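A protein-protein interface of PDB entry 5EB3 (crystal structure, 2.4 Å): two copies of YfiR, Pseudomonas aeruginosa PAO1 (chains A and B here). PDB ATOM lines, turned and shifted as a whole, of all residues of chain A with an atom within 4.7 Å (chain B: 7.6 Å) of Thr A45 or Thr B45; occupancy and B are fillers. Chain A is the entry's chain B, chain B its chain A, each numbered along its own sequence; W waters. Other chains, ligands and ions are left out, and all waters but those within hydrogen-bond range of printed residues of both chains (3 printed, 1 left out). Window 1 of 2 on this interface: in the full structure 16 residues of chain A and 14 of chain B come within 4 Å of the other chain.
The backbone NH (N) of Thr B45 lies within hydrogen-bond range of the backbone carbonyl oxygen (O) of Thr A45, at 3.1 Å.
The side-chain carboxylate (OD2) of Asp B49 is in salt-bridge range of the guanidinium group (NE) of Arg A67, 2.4 Å away.
The guanidinium group of Arg B67 sits at hydrogen-bond distance from the backbone carbonyl oxygen of Thr A45 (3.2 Å).
The guanidinium group of Arg B67 lies close to the backbone carbonyl oxygen of Glu A46, 3.4 Å away.
The backbone carbonyl oxygen (O) of Pro B44 sits at hydrogen-bond distance from the backbone NH (N) of Val B86, 2.8 Å away.
The backbone NH of Glu B46 lies within hydrogen-bond range of the side-chain carboxylate of Glu B109 (2.8 Å).
NH2 of Arg B110 lies within salt-bridge range of OE2 of Glu B46 (3.99 Å).
OG1 of Thr A45 is in hydrogen-bond range of NH1 of Arg A67 (3.1 Å).
N of Glu A46 lies within hydrogen-bond range of OE2 of Glu A109 (2.8 Å).
Glu B46 touches Gly A43 (OE1 to CA, 3.7 Å).
Pro A44 touches Pro B44.
Thr B45 touches Pro A44.
Pro A44 touches Glu B46.
Pro A44 touches Val B86 (CG to CG2, 3.9 Å).
CG of Pro A44 touches NH2 of Arg B110, at 3.4 Å.
Pro B44 touches Thr A45.
Glu A46 touches Gly B43.
CG of Glu A46 touches N of Pro B44, at 3.5 Å.
NH1 of Arg A67 touches O of Thr B45, 3.6 Å away.
Thr A45 touches just these residues of chain B: Pro B44 (3.5 Å), Thr B45 (3.1 Å) and Arg B67 (3.2 Å).
Of the printed residues of chain A, Asp B49 touches Arg A67 (2.4 Å).
Printed residues of chain A within 4 Å of Arg B67: Thr A45 and Glu A46.
Leu B84 touches none of the printed residues of chain A.
The nearest residue of chain A that does not touch Thr B45 is Gly A43 (4.6 Å).
Of the 11 printed residues of chain A, 5 touch a printed residue of chain B.
Hydrophobic or aromatic side chains of chain A within 4 Å of the printed part of chain B: Pro A44.
Along chain A the printed residues that touch a printed residue of chain B span positions 43 to 67.
Printed residues of chain B that touch a printed residue of chain A: Gly B43, Pro B44, Thr B45, Glu B46, Asp B49, Arg B67, Val B86 and Arg B110.
Hydrophobic or aromatic side chains of chain B within 4 Å of the printed part of chain A: Pro B44 and Val B86.
Among the printed residues, Asp or Glu carboxylates within 4 Å of a Lys or Arg side-chain nitrogen of the other chain: Arg A67 with Asp B49.
Pro A44 touches its own counterpart, Pro B44.
Pro A44 touches Thr B45, and with the chains exchanged Thr A45 touches Pro B44.
Pro A44 touches Glu B46, and with the chains exchanged Glu A46 touches Pro B44.
Thr A45 touches its own counterpart, Thr B45.
Of the 15 pairs that touch across the chains among the printed residues, 12 have their exchanged pair printed and touching as well.
Water W2 lies within hydrogen-bond range of the side-chain carboxylate of Asp B49, the backbone NH of Ala B48, the side-chain hydroxyl of Thr B45 and the guanidinium group of Arg A67.
Water W3 lies within hydrogen-bond range of the side-chain carboxylate of Glu B46 (2.7 Å) and the backbone NH of Gly A43 (2.9 Å).
Water W1 lies within hydrogen-bond range of OE1 of Glu A46 and N of Gly B43.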
ATOM      1  N   VAL A  41      13.303   0.520 -13.224  1.00  0.00           N
ATOM      2  CA  VAL A  41      13.688  -0.267 -12.057  1.00  0.00           C
ATOM      3  C   VAL A  41      14.285  -1.572 -12.558  1.00  0.00           C
ATOM      4  O   VAL A  41      13.619  -2.332 -13.274  1.00  0.00           O
ATOM      5  CB  VAL A  41      12.482  -0.567 -11.183  1.00  0.00           C
ATOM      6  CG1 VAL A  41      12.908  -1.313  -9.926  1.00  0.00           C
ATOM      7  CG2 VAL A  41      11.776   0.730 -10.836  1.00  0.00           C
ATOM      8  N   GLY A  43      16.438  -5.125 -11.772  1.00  0.00           N
ATOM      9  CA  GLY A  43      16.839  -6.096 -10.773  1.00  0.00           C
ATOM     10  C   GLY A  43      15.887  -6.092  -9.597  1.00  0.00           C
ATOM     11  O   GLY A  43      15.013  -5.224  -9.518  1.00  0.00           O
ATOM     12  N   PRO A  44      16.051  -7.060  -8.675  1.00  0.00           N
ATOM     13  CA  PRO A  44      15.209  -7.224  -7.485  1.00  0.00           C
ATOM     14  C   PRO A  44      15.279  -6.010  -6.579  1.00  0.00           C
ATOM     15  O   PRO A  44      16.378  -5.571  -6.274  1.00  0.00           O
ATOM     16  CB  PRO A  44      15.855  -8.415  -6.765  1.00  0.00           C
ATOM     17  CG  PRO A  44      16.567  -9.175  -7.832  1.00  0.00           C
ATOM     18  CD  PRO A  44      17.079  -8.111  -8.769  1.00  0.00           C
ATOM     19  N   THR A  45      14.130  -5.494  -6.147  1.00  0.00           N
ATOM     20  CA  THR A  45      14.078  -4.329  -5.265  1.00  0.00           C
ATOM     21  C   THR A  45      13.084  -4.521  -4.136  1.00  0.00           C
ATOM     22  O   THR A  45      12.081  -5.205  -4.295  1.00  0.00           O
ATOM     23  CB  THR A  45      13.658  -3.062  -6.031  1.00  0.00           C
ATOM     24  OG1 THR A  45      12.402  -3.285  -6.690  1.00  0.00           O
ATOM     25  CG2 THR A  45      14.710  -2.672  -7.058  1.00  0.00           C
ATOM     26  N   GLU A  46      13.354  -3.902  -2.996  1.00  0.00           N
ATOM     27  CA  GLU A  46      12.432  -3.966  -1.865  1.00  0.00           C
ATOM     28  C   GLU A  46      11.541  -2.740  -1.809  1.00  0.00           C
ATOM     29  O   GLU A  46      10.410  -2.793  -1.322  1.00  0.00           O
ATOM     30  CB  GLU A  46      13.214  -3.995  -0.557  1.00  0.00           C
ATOM     31  CG  GLU A  46      13.102  -5.259   0.229  1.00  0.00           C
ATOM     32  CD  GLU A  46      13.869  -5.182   1.525  1.00  0.00           C
ATOM     33  OE1 GLU A  46      13.273  -5.521   2.565  1.00  0.00           O
ATOM     34  OE2 GLU A  46      15.059  -4.786   1.505  1.00  0.00           O
ATOM     35  N   TYR A  47      12.070  -1.618  -2.282  1.00  0.00           N
ATOM     36  CA  TYR A  47      11.470  -0.343  -1.960  1.00  0.00           C
ATOM     37  C   TYR A  47      11.029   0.453  -3.198  1.00  0.00           C
ATOM     38  O   TYR A  47      10.830   1.674  -3.133  1.00  0.00           O
ATOM     39  CB  TYR A  47      12.456   0.466  -1.115  1.00  0.00           C
ATOM     40  CG  TYR A  47      12.905  -0.191   0.178  1.00  0.00           C
ATOM     41  CD1 TYR A  47      12.070  -0.250   1.290  1.00  0.00           C
ATOM     42  CD2 TYR A  47      14.189  -0.702   0.304  1.00  0.00           C
ATOM     43  CE1 TYR A  47      12.498  -0.832   2.479  1.00  0.00           C
ATOM     44  CE2 TYR A  47      14.624  -1.286   1.485  1.00  0.00           C
ATOM     45  CZ  TYR A  47      13.780  -1.347   2.566  1.00  0.00           C
ATOM     46  OH  TYR A  47      14.224  -1.924   3.740  1.00  0.00           O
ATOM     47  N   ALA A  48      10.855  -0.228  -4.324  1.00  0.00           N
ATOM     48  CA  ALA A  48      10.523   0.491  -5.552  1.00  0.00           C
ATOM     49  C   ALA A  48       9.024   0.593  -5.846  1.00  0.00           C
ATOM     50  O   ALA A  48       8.643   1.216  -6.843  1.00  0.00           O
ATOM     51  CB  ALA A  48      11.265  -0.102  -6.741  1.00  0.00           C
ATOM     52  N   ARG A  67       9.577  -1.945 -14.605  1.00  0.00           N
ATOM     53  CA  ARG A  67      10.731  -2.811 -14.461  1.00  0.00           C
ATOM     54  C   ARG A  67      11.244  -3.163 -15.841  1.00  0.00           C
ATOM     55  O   ARG A  67      10.459  -3.429 -16.756  1.00  0.00           O
ATOM     56  CB  ARG A  67      10.375  -4.081 -13.693  1.00  0.00           C
ATOM     57  CG  ARG A  67       9.988  -3.823 -12.254  1.00  0.00           C
ATOM     58  CD  ARG A  67       9.754  -5.116 -11.498  1.00  0.00           C
ATOM     59  NE  ARG A  67       9.250  -4.826 -10.167  1.00  0.00           N
ATOM     60  CZ  ARG A  67      10.033  -4.537  -9.134  1.00  0.00           C
ATOM     61  NH1 ARG A  67      11.354  -4.518  -9.294  1.00  0.00           N
ATOM     62  NH2 ARG A  67       9.500  -4.266  -7.942  1.00  0.00           N
ATOM     63  N   TYR A  83      16.947   2.878 -11.429  1.00  0.00           N
ATOM     64  CA  TYR A  83      16.941   2.586 -10.013  1.00  0.00           C
ATOM     65  C   TYR A  83      17.340   1.124  -9.880  1.00  0.00           C
ATOM     66  O   TYR A  83      16.559   0.220 -10.183  1.00  0.00           O
ATOM     67  CB  TYR A  83      15.569   2.881  -9.412  1.00  0.00           C
ATOM     68  CG  TYR A  83      15.451   2.553  -7.941  1.00  0.00           C
ATOM     69  CD1 TYR A  83      15.818   3.472  -6.965  1.00  0.00           C
ATOM     70  CD2 TYR A  83      14.967   1.324  -7.532  1.00  0.00           C
ATOM     71  CE1 TYR A  83      15.709   3.166  -5.620  1.00  0.00           C
ATOM     72  CE2 TYR A  83      14.852   1.008  -6.196  1.00  0.00           C
ATOM     73  CZ  TYR A  83      15.222   1.929  -5.248  1.00  0.00           C
ATOM     74  OH  TYR A  83      15.093   1.610  -3.925  1.00  0.00           O
ATOM     75  N   GLY A  85      18.572  -2.419  -8.393  1.00  0.00           N
ATOM     76  CA  GLY A  85      18.433  -3.301  -7.243  1.00  0.00           C
ATOM     77  C   GLY A  85      19.582  -4.291  -7.157  1.00  0.00           C
ATOM     78  O   GLY A  85      20.716  -3.969  -7.522  1.00  0.00           O
ATOM     79  N   GLU A 109      19.614   0.948  -4.862  1.00  0.00           N
ATOM     80  CA  GLU A 109      18.829   0.806  -3.633  1.00  0.00           C
ATOM     81  C   GLU A 109      19.694   0.423  -2.425  1.00  0.00           C
ATOM     82  O   GLU A 109      19.453   0.890  -1.300  1.00  0.00           O
ATOM     83  CB  GLU A 109      17.693  -0.211  -3.845  1.00  0.00           C
ATOM     84  CG  GLU A 109      16.972  -0.639  -2.579  1.00  0.00           C
ATOM     85  CD  GLU A 109      15.806  -1.562  -2.861  1.00  0.00           C
ATOM     86  OE1 GLU A 109      14.753  -1.060  -3.313  1.00  0.00           O
ATOM     87  OE2 GLU A 109      15.937  -2.786  -2.627  1.00  0.00           O
ATOM     88  N   VAL B  41       5.692 -10.788   1.076  1.00  0.00           N
ATOM     89  CA  VAL B  41       6.853 -10.716   0.198  1.00  0.00           C
ATOM     90  C   VAL B  41       7.995 -10.163   1.044  1.00  0.00           C
ATOM     91  O   VAL B  41       7.862  -9.105   1.674  1.00  0.00           O
ATOM     92  CB  VAL B  41       6.581  -9.818  -1.021  1.00  0.00           C
ATOM     93  CG1 VAL B  41       7.832  -9.639  -1.834  1.00  0.00           C
ATOM     94  CG2 VAL B  41       5.490 -10.422  -1.884  1.00  0.00           C
ATOM     95  N   VAL B  42       9.103 -10.895   1.093  1.00  0.00           N
ATOM     96  CA  VAL B  42      10.187 -10.554   2.000  1.00  0.00           C
ATOM     97  C   VAL B  42      11.523 -10.449   1.274  1.00  0.00           C
ATOM     98  O   VAL B  42      11.982 -11.413   0.653  1.00  0.00           O
ATOM     99  CB  VAL B  42      10.303 -11.598   3.126  1.00  0.00           C
ATOM    100  CG1 VAL B  42      11.463 -11.260   4.037  1.00  0.00           C
ATOM    101  CG2 VAL B  42       9.031 -11.639   3.921  1.00  0.00           C
ATOM    102  N   GLY B  43      12.152  -9.282   1.365  1.00  0.00           N
ATOM    103  CA  GLY B  43      13.415  -9.061   0.684  1.00  0.00           C
ATOM    104  C   GLY B  43      13.167  -8.524  -0.710  1.00  0.00           C
ATOM    105  O   GLY B  43      12.018  -8.439  -1.138  1.00  0.00           O
ATOM    106  N   PRO B  44      14.245  -8.147  -1.421  1.00  0.00           N
ATOM    107  CA  PRO B  44      14.148  -7.597  -2.780  1.00  0.00           C
ATOM    108  C   PRO B  44      13.598  -8.624  -3.763  1.00  0.00           C
ATOM    109  O   PRO B  44      14.099  -9.751  -3.803  1.00  0.00           O
ATOM    110  CB  PRO B  44      15.603  -7.290  -3.143  1.00  0.00           C
ATOM    111  CG  PRO B  44      16.334  -7.214  -1.820  1.00  0.00           C
ATOM    112  CD  PRO B  44      15.633  -8.174  -0.918  1.00  0.00           C
ATOM    113  N   THR B  45      12.593  -8.237  -4.544  1.00  0.00           N
ATOM    114  CA  THR B  45      12.012  -9.123  -5.549  1.00  0.00           C
ATOM    115  C   THR B  45      11.888  -8.424  -6.896  1.00  0.00           C
ATOM    116  O   THR B  45      11.691  -7.216  -6.980  1.00  0.00           O
ATOM    117  CB  THR B  45      10.612  -9.583  -5.148  1.00  0.00           C
ATOM    118  OG1 THR B  45       9.781  -8.429  -4.954  1.00  0.00           O
ATOM    119  CG2 THR B  45      10.658 -10.406  -3.865  1.00  0.00           C
ATOM    120  N   GLU B  46      11.980  -9.204  -7.955  1.00  0.00           N
ATOM    121  CA  GLU B  46      11.926  -8.661  -9.291  1.00  0.00           C
ATOM    122  C   GLU B  46      10.572  -9.017  -9.929  1.00  0.00           C
ATOM    123  O   GLU B  46      10.093  -8.326 -10.832  1.00  0.00           O
ATOM    124  CB  GLU B  46      13.087  -9.257 -10.088  1.00  0.00           C
ATOM    125  CG  GLU B  46      13.426  -8.546 -11.377  1.00  0.00           C
ATOM    126  CD  GLU B  46      14.683  -9.099 -12.008  1.00  0.00           C
ATOM    127  OE1 GLU B  46      15.124  -8.521 -13.022  1.00  0.00           O
ATOM    128  OE2 GLU B  46      15.226 -10.111 -11.491  1.00  0.00           O
ATOM    129  N   TYR B  47       9.944 -10.082  -9.428  1.00  0.00           N
ATOM    130  CA  TYR B  47       8.776 -10.668 -10.087  1.00  0.00           C
ATOM    131  C   TYR B  47       7.525 -10.751  -9.216  1.00  0.00           C
ATOM    132  O   TYR B  47       6.638 -11.559  -9.492  1.00  0.00           O
ATOM    133  CB  TYR B  47       9.132 -12.068 -10.575  1.00  0.00           C
ATOM    134  CG  TYR B  47      10.274 -12.076 -11.568  1.00  0.00           C
ATOM    135  CD1 TYR B  47      10.129 -11.496 -12.825  1.00  0.00           C
ATOM    136  CD2 TYR B  47      11.485 -12.676 -11.258  1.00  0.00           C
ATOM    137  CE1 TYR B  47      11.165 -11.509 -13.744  1.00  0.00           C
ATOM    138  CE2 TYR B  47      12.529 -12.689 -12.172  1.00  0.00           C
ATOM    139  CZ  TYR B  47      12.359 -12.106 -13.414  1.00  0.00           C
ATOM    140  OH  TYR B  47      13.386 -12.123 -14.334  1.00  0.00           O
ATOM    141  N   ALA B  48       7.446  -9.907  -8.187  1.00  0.00           N
ATOM    142  CA  ALA B  48       6.394 -10.033  -7.183  1.00  0.00           C
ATOM    143  C   ALA B  48       5.327  -8.952  -7.317  1.00  0.00           C
ATOM    144  O   ALA B  48       4.380  -8.908  -6.518  1.00  0.00           O
ATOM    145  CB  ALA B  48       6.993 -10.004  -5.798  1.00  0.00           C
ATOM    146  N   ASP B  49       5.471  -8.087  -8.319  1.00  0.00           N
ATOM    147  CA  ASP B  49       4.541  -6.971  -8.477  1.00  0.00           C
ATOM    148  C   ASP B  49       3.126  -7.456  -8.748  1.00  0.00           C
ATOM    149  O   ASP B  49       2.159  -6.837  -8.297  1.00  0.00           O
ATOM    150  CB  ASP B  49       4.996  -6.009  -9.573  1.00  0.00           C
ATOM    151  CG  ASP B  49       6.260  -5.273  -9.202  1.00  0.00           C
ATOM    152  OD1 ASP B  49       6.675  -5.373  -8.026  1.00  0.00           O
ATOM    153  OD2 ASP B  49       6.834  -4.587 -10.077  1.00  0.00           O
ATOM    154  N   LEU B  51       1.821 -10.548  -7.651  1.00  0.00           N
ATOM    155  CA  LEU B  51       1.374 -11.028  -6.334  1.00  0.00           C
ATOM    156  C   LEU B  51       0.863  -9.870  -5.490  1.00  0.00           C
ATOM    157  O   LEU B  51      -0.180  -9.960  -4.839  1.00  0.00           O
ATOM    158  CB  LEU B  51       2.535 -11.641  -5.559  1.00  0.00           C
ATOM    159  CG  LEU B  51       3.420 -12.647  -6.274  1.00  0.00           C
ATOM    160  CD1 LEU B  51       4.472 -13.220  -5.326  1.00  0.00           C
ATOM    161  CD2 LEU B  51       2.542 -13.741  -6.834  1.00  0.00           C
ATOM    162  N   LEU B  52       1.614  -8.774  -5.501  1.00  0.00           N
ATOM    163  CA  LEU B  52       1.311  -7.668  -4.602  1.00  0.00           C
ATOM    164  C   LEU B  52       0.000  -6.937  -4.936  1.00  0.00           C
ATOM    165  O   LEU B  52      -0.503  -6.162  -4.125  1.00  0.00           O
ATOM    166  CB  LEU B  52       2.493  -6.709  -4.520  1.00  0.00           C
ATOM    167  CG  LEU B  52       3.653  -7.219  -3.670  1.00  0.00           C
ATOM    168  CD1 LEU B  52       4.897  -6.405  -3.945  1.00  0.00           C
ATOM    169  CD2 LEU B  52       3.303  -7.177  -2.182  1.00  0.00           C
ATOM    170  N   ARG B  67       4.534  -6.436   1.262  1.00  0.00           N
ATOM    171  CA  ARG B  67       5.937  -6.627   1.592  1.00  0.00           C
ATOM    172  C   ARG B  67       6.106  -6.463   3.096  1.00  0.00           C
ATOM    173  O   ARG B  67       5.425  -5.646   3.723  1.00  0.00           O
ATOM    174  CB  ARG B  67       6.838  -5.624   0.857  1.00  0.00           C
ATOM    175  CG  ARG B  67       6.370  -5.222  -0.522  1.00  0.00           C
ATOM    176  CD  ARG B  67       7.496  -4.549  -1.301  1.00  0.00           C
ATOM    177  NE  ARG B  67       8.429  -5.543  -1.809  1.00  0.00           N
ATOM    178  CZ  ARG B  67       8.584  -5.842  -3.096  1.00  0.00           C
ATOM    179  NH1 ARG B  67       7.887  -5.198  -4.036  1.00  0.00           N
ATOM    180  NH2 ARG B  67       9.461  -6.782  -3.440  1.00  0.00           N
ATOM    181  N   TYR B  83       6.778 -15.271   0.189  1.00  0.00           N
ATOM    182  CA  TYR B  83       7.478 -15.244  -1.084  1.00  0.00           C
ATOM    183  C   TYR B  83       8.845 -14.637  -0.778  1.00  0.00           C
ATOM    184  O   TYR B  83       8.961 -13.439  -0.499  1.00  0.00           O
ATOM    185  CB  TYR B  83       6.700 -14.425  -2.112  1.00  0.00           C
ATOM    186  CG  TYR B  83       7.334 -14.369  -3.481  1.00  0.00           C
ATOM    187  CD1 TYR B  83       7.118 -15.376  -4.405  1.00  0.00           C
ATOM    188  CD2 TYR B  83       8.137 -13.298  -3.857  1.00  0.00           C
ATOM    189  CE1 TYR B  83       7.692 -15.328  -5.669  1.00  0.00           C
ATOM    190  CE2 TYR B  83       8.716 -13.241  -5.121  1.00  0.00           C
ATOM    191  CZ  TYR B  83       8.489 -14.262  -6.016  1.00  0.00           C
ATOM    192  OH  TYR B  83       9.053 -14.226  -7.273  1.00  0.00           O
ATOM    193  N   LEU B  84       9.876 -15.477  -0.782  1.00  0.00           N
ATOM    194  CA  LEU B  84      11.208 -15.037  -0.385  1.00  0.00           C
ATOM    195  C   LEU B  84      11.997 -14.442  -1.550  1.00  0.00           C
ATOM    196  O   LEU B  84      12.169 -15.066  -2.606  1.00  0.00           O
ATOM    197  CB  LEU B  84      11.988 -16.186   0.265  1.00  0.00           C
ATOM    198  CG  LEU B  84      13.376 -15.861   0.829  1.00  0.00           C
ATOM    199  CD1 LEU B  84      13.290 -14.868   1.976  1.00  0.00           C
ATOM    200  CD2 LEU B  84      14.093 -17.129   1.272  1.00  0.00           C
ATOM    201  N   GLY B  85      12.475 -13.223  -1.346  1.00  0.00           N
ATOM    202  CA  GLY B  85      13.268 -12.546  -2.350  1.00  0.00           C
ATOM    203  C   GLY B  85      14.749 -12.841  -2.209  1.00  0.00           C
ATOM    204  O   GLY B  85      15.139 -13.849  -1.612  1.00  0.00           O
ATOM    205  N   VAL B  86      15.571 -11.951  -2.758  1.00  0.00           N
ATOM    206  CA  VAL B  86      17.009 -12.176  -2.831  1.00  0.00           C
ATOM    207  C   VAL B  86      17.712 -11.533  -1.642  1.00  0.00           C
ATOM    208  O   VAL B  86      18.113 -10.370  -1.697  1.00  0.00           O
ATOM    209  CB  VAL B  86      17.569 -11.646  -4.159  1.00  0.00           C
ATOM    210  CG1 VAL B  86      19.020 -12.011  -4.308  1.00  0.00           C
ATOM    211  CG2 VAL B  86      16.761 -12.218  -5.326  1.00  0.00           C
ATOM    212  N   GLU B 109      11.880 -16.675  -4.984  1.00  0.00           N
ATOM    213  CA  GLU B 109      11.931 -16.173  -6.346  1.00  0.00           C
ATOM    214  C   GLU B 109      13.082 -16.820  -7.114  1.00  0.00           C
ATOM    215  O   GLU B 109      13.010 -16.985  -8.336  1.00  0.00           O
ATOM    216  CB  GLU B 109      12.078 -14.655  -6.349  1.00  0.00           C
ATOM    217  CG  GLU B 109      12.171 -14.071  -7.737  1.00  0.00           C
ATOM    218  CD  GLU B 109      11.984 -12.583  -7.740  1.00  0.00           C
ATOM    219  OE1 GLU B 109      10.811 -12.147  -7.712  1.00  0.00           O
ATOM    220  OE2 GLU B 109      13.004 -11.856  -7.781  1.00  0.00           O
ATOM    221  N   ARG B 110      14.134 -17.211  -6.392  1.00  0.00           N
ATOM    222  CA  ARG B 110      15.302 -17.816  -7.036  1.00  0.00           C
ATOM    223  C   ARG B 110      15.565 -19.258  -6.605  1.00  0.00           C
ATOM    224  O   ARG B 110      15.233 -19.642  -5.478  1.00  0.00           O
ATOM    225  CB  ARG B 110      16.531 -16.937  -6.826  1.00  0.00           C
ATOM    226  CG  ARG B 110      16.394 -15.633  -7.563  1.00  0.00           C
ATOM    227  CD  ARG B 110      17.690 -14.880  -7.644  1.00  0.00           C
ATOM    228  NE  ARG B 110      17.512 -13.668  -8.438  1.00  0.00           N
ATOM    229  CZ  ARG B 110      18.472 -12.782  -8.658  1.00  0.00           C
ATOM    230  NH1 ARG B 110      19.676 -12.974  -8.135  1.00  0.00           N
ATOM    231  NH2 ARG B 110      18.226 -11.705  -9.392  1.00  0.00           N
HETATM  232  O   HOH W   1      10.544  -6.639   2.281  1.00  0.00           O
HETATM  233  O   HOH W   2       8.479  -7.255  -7.396  1.00  0.00           O
HETATM  234  O   HOH W   3      14.140  -5.968 -13.250  1.00  0.00           O
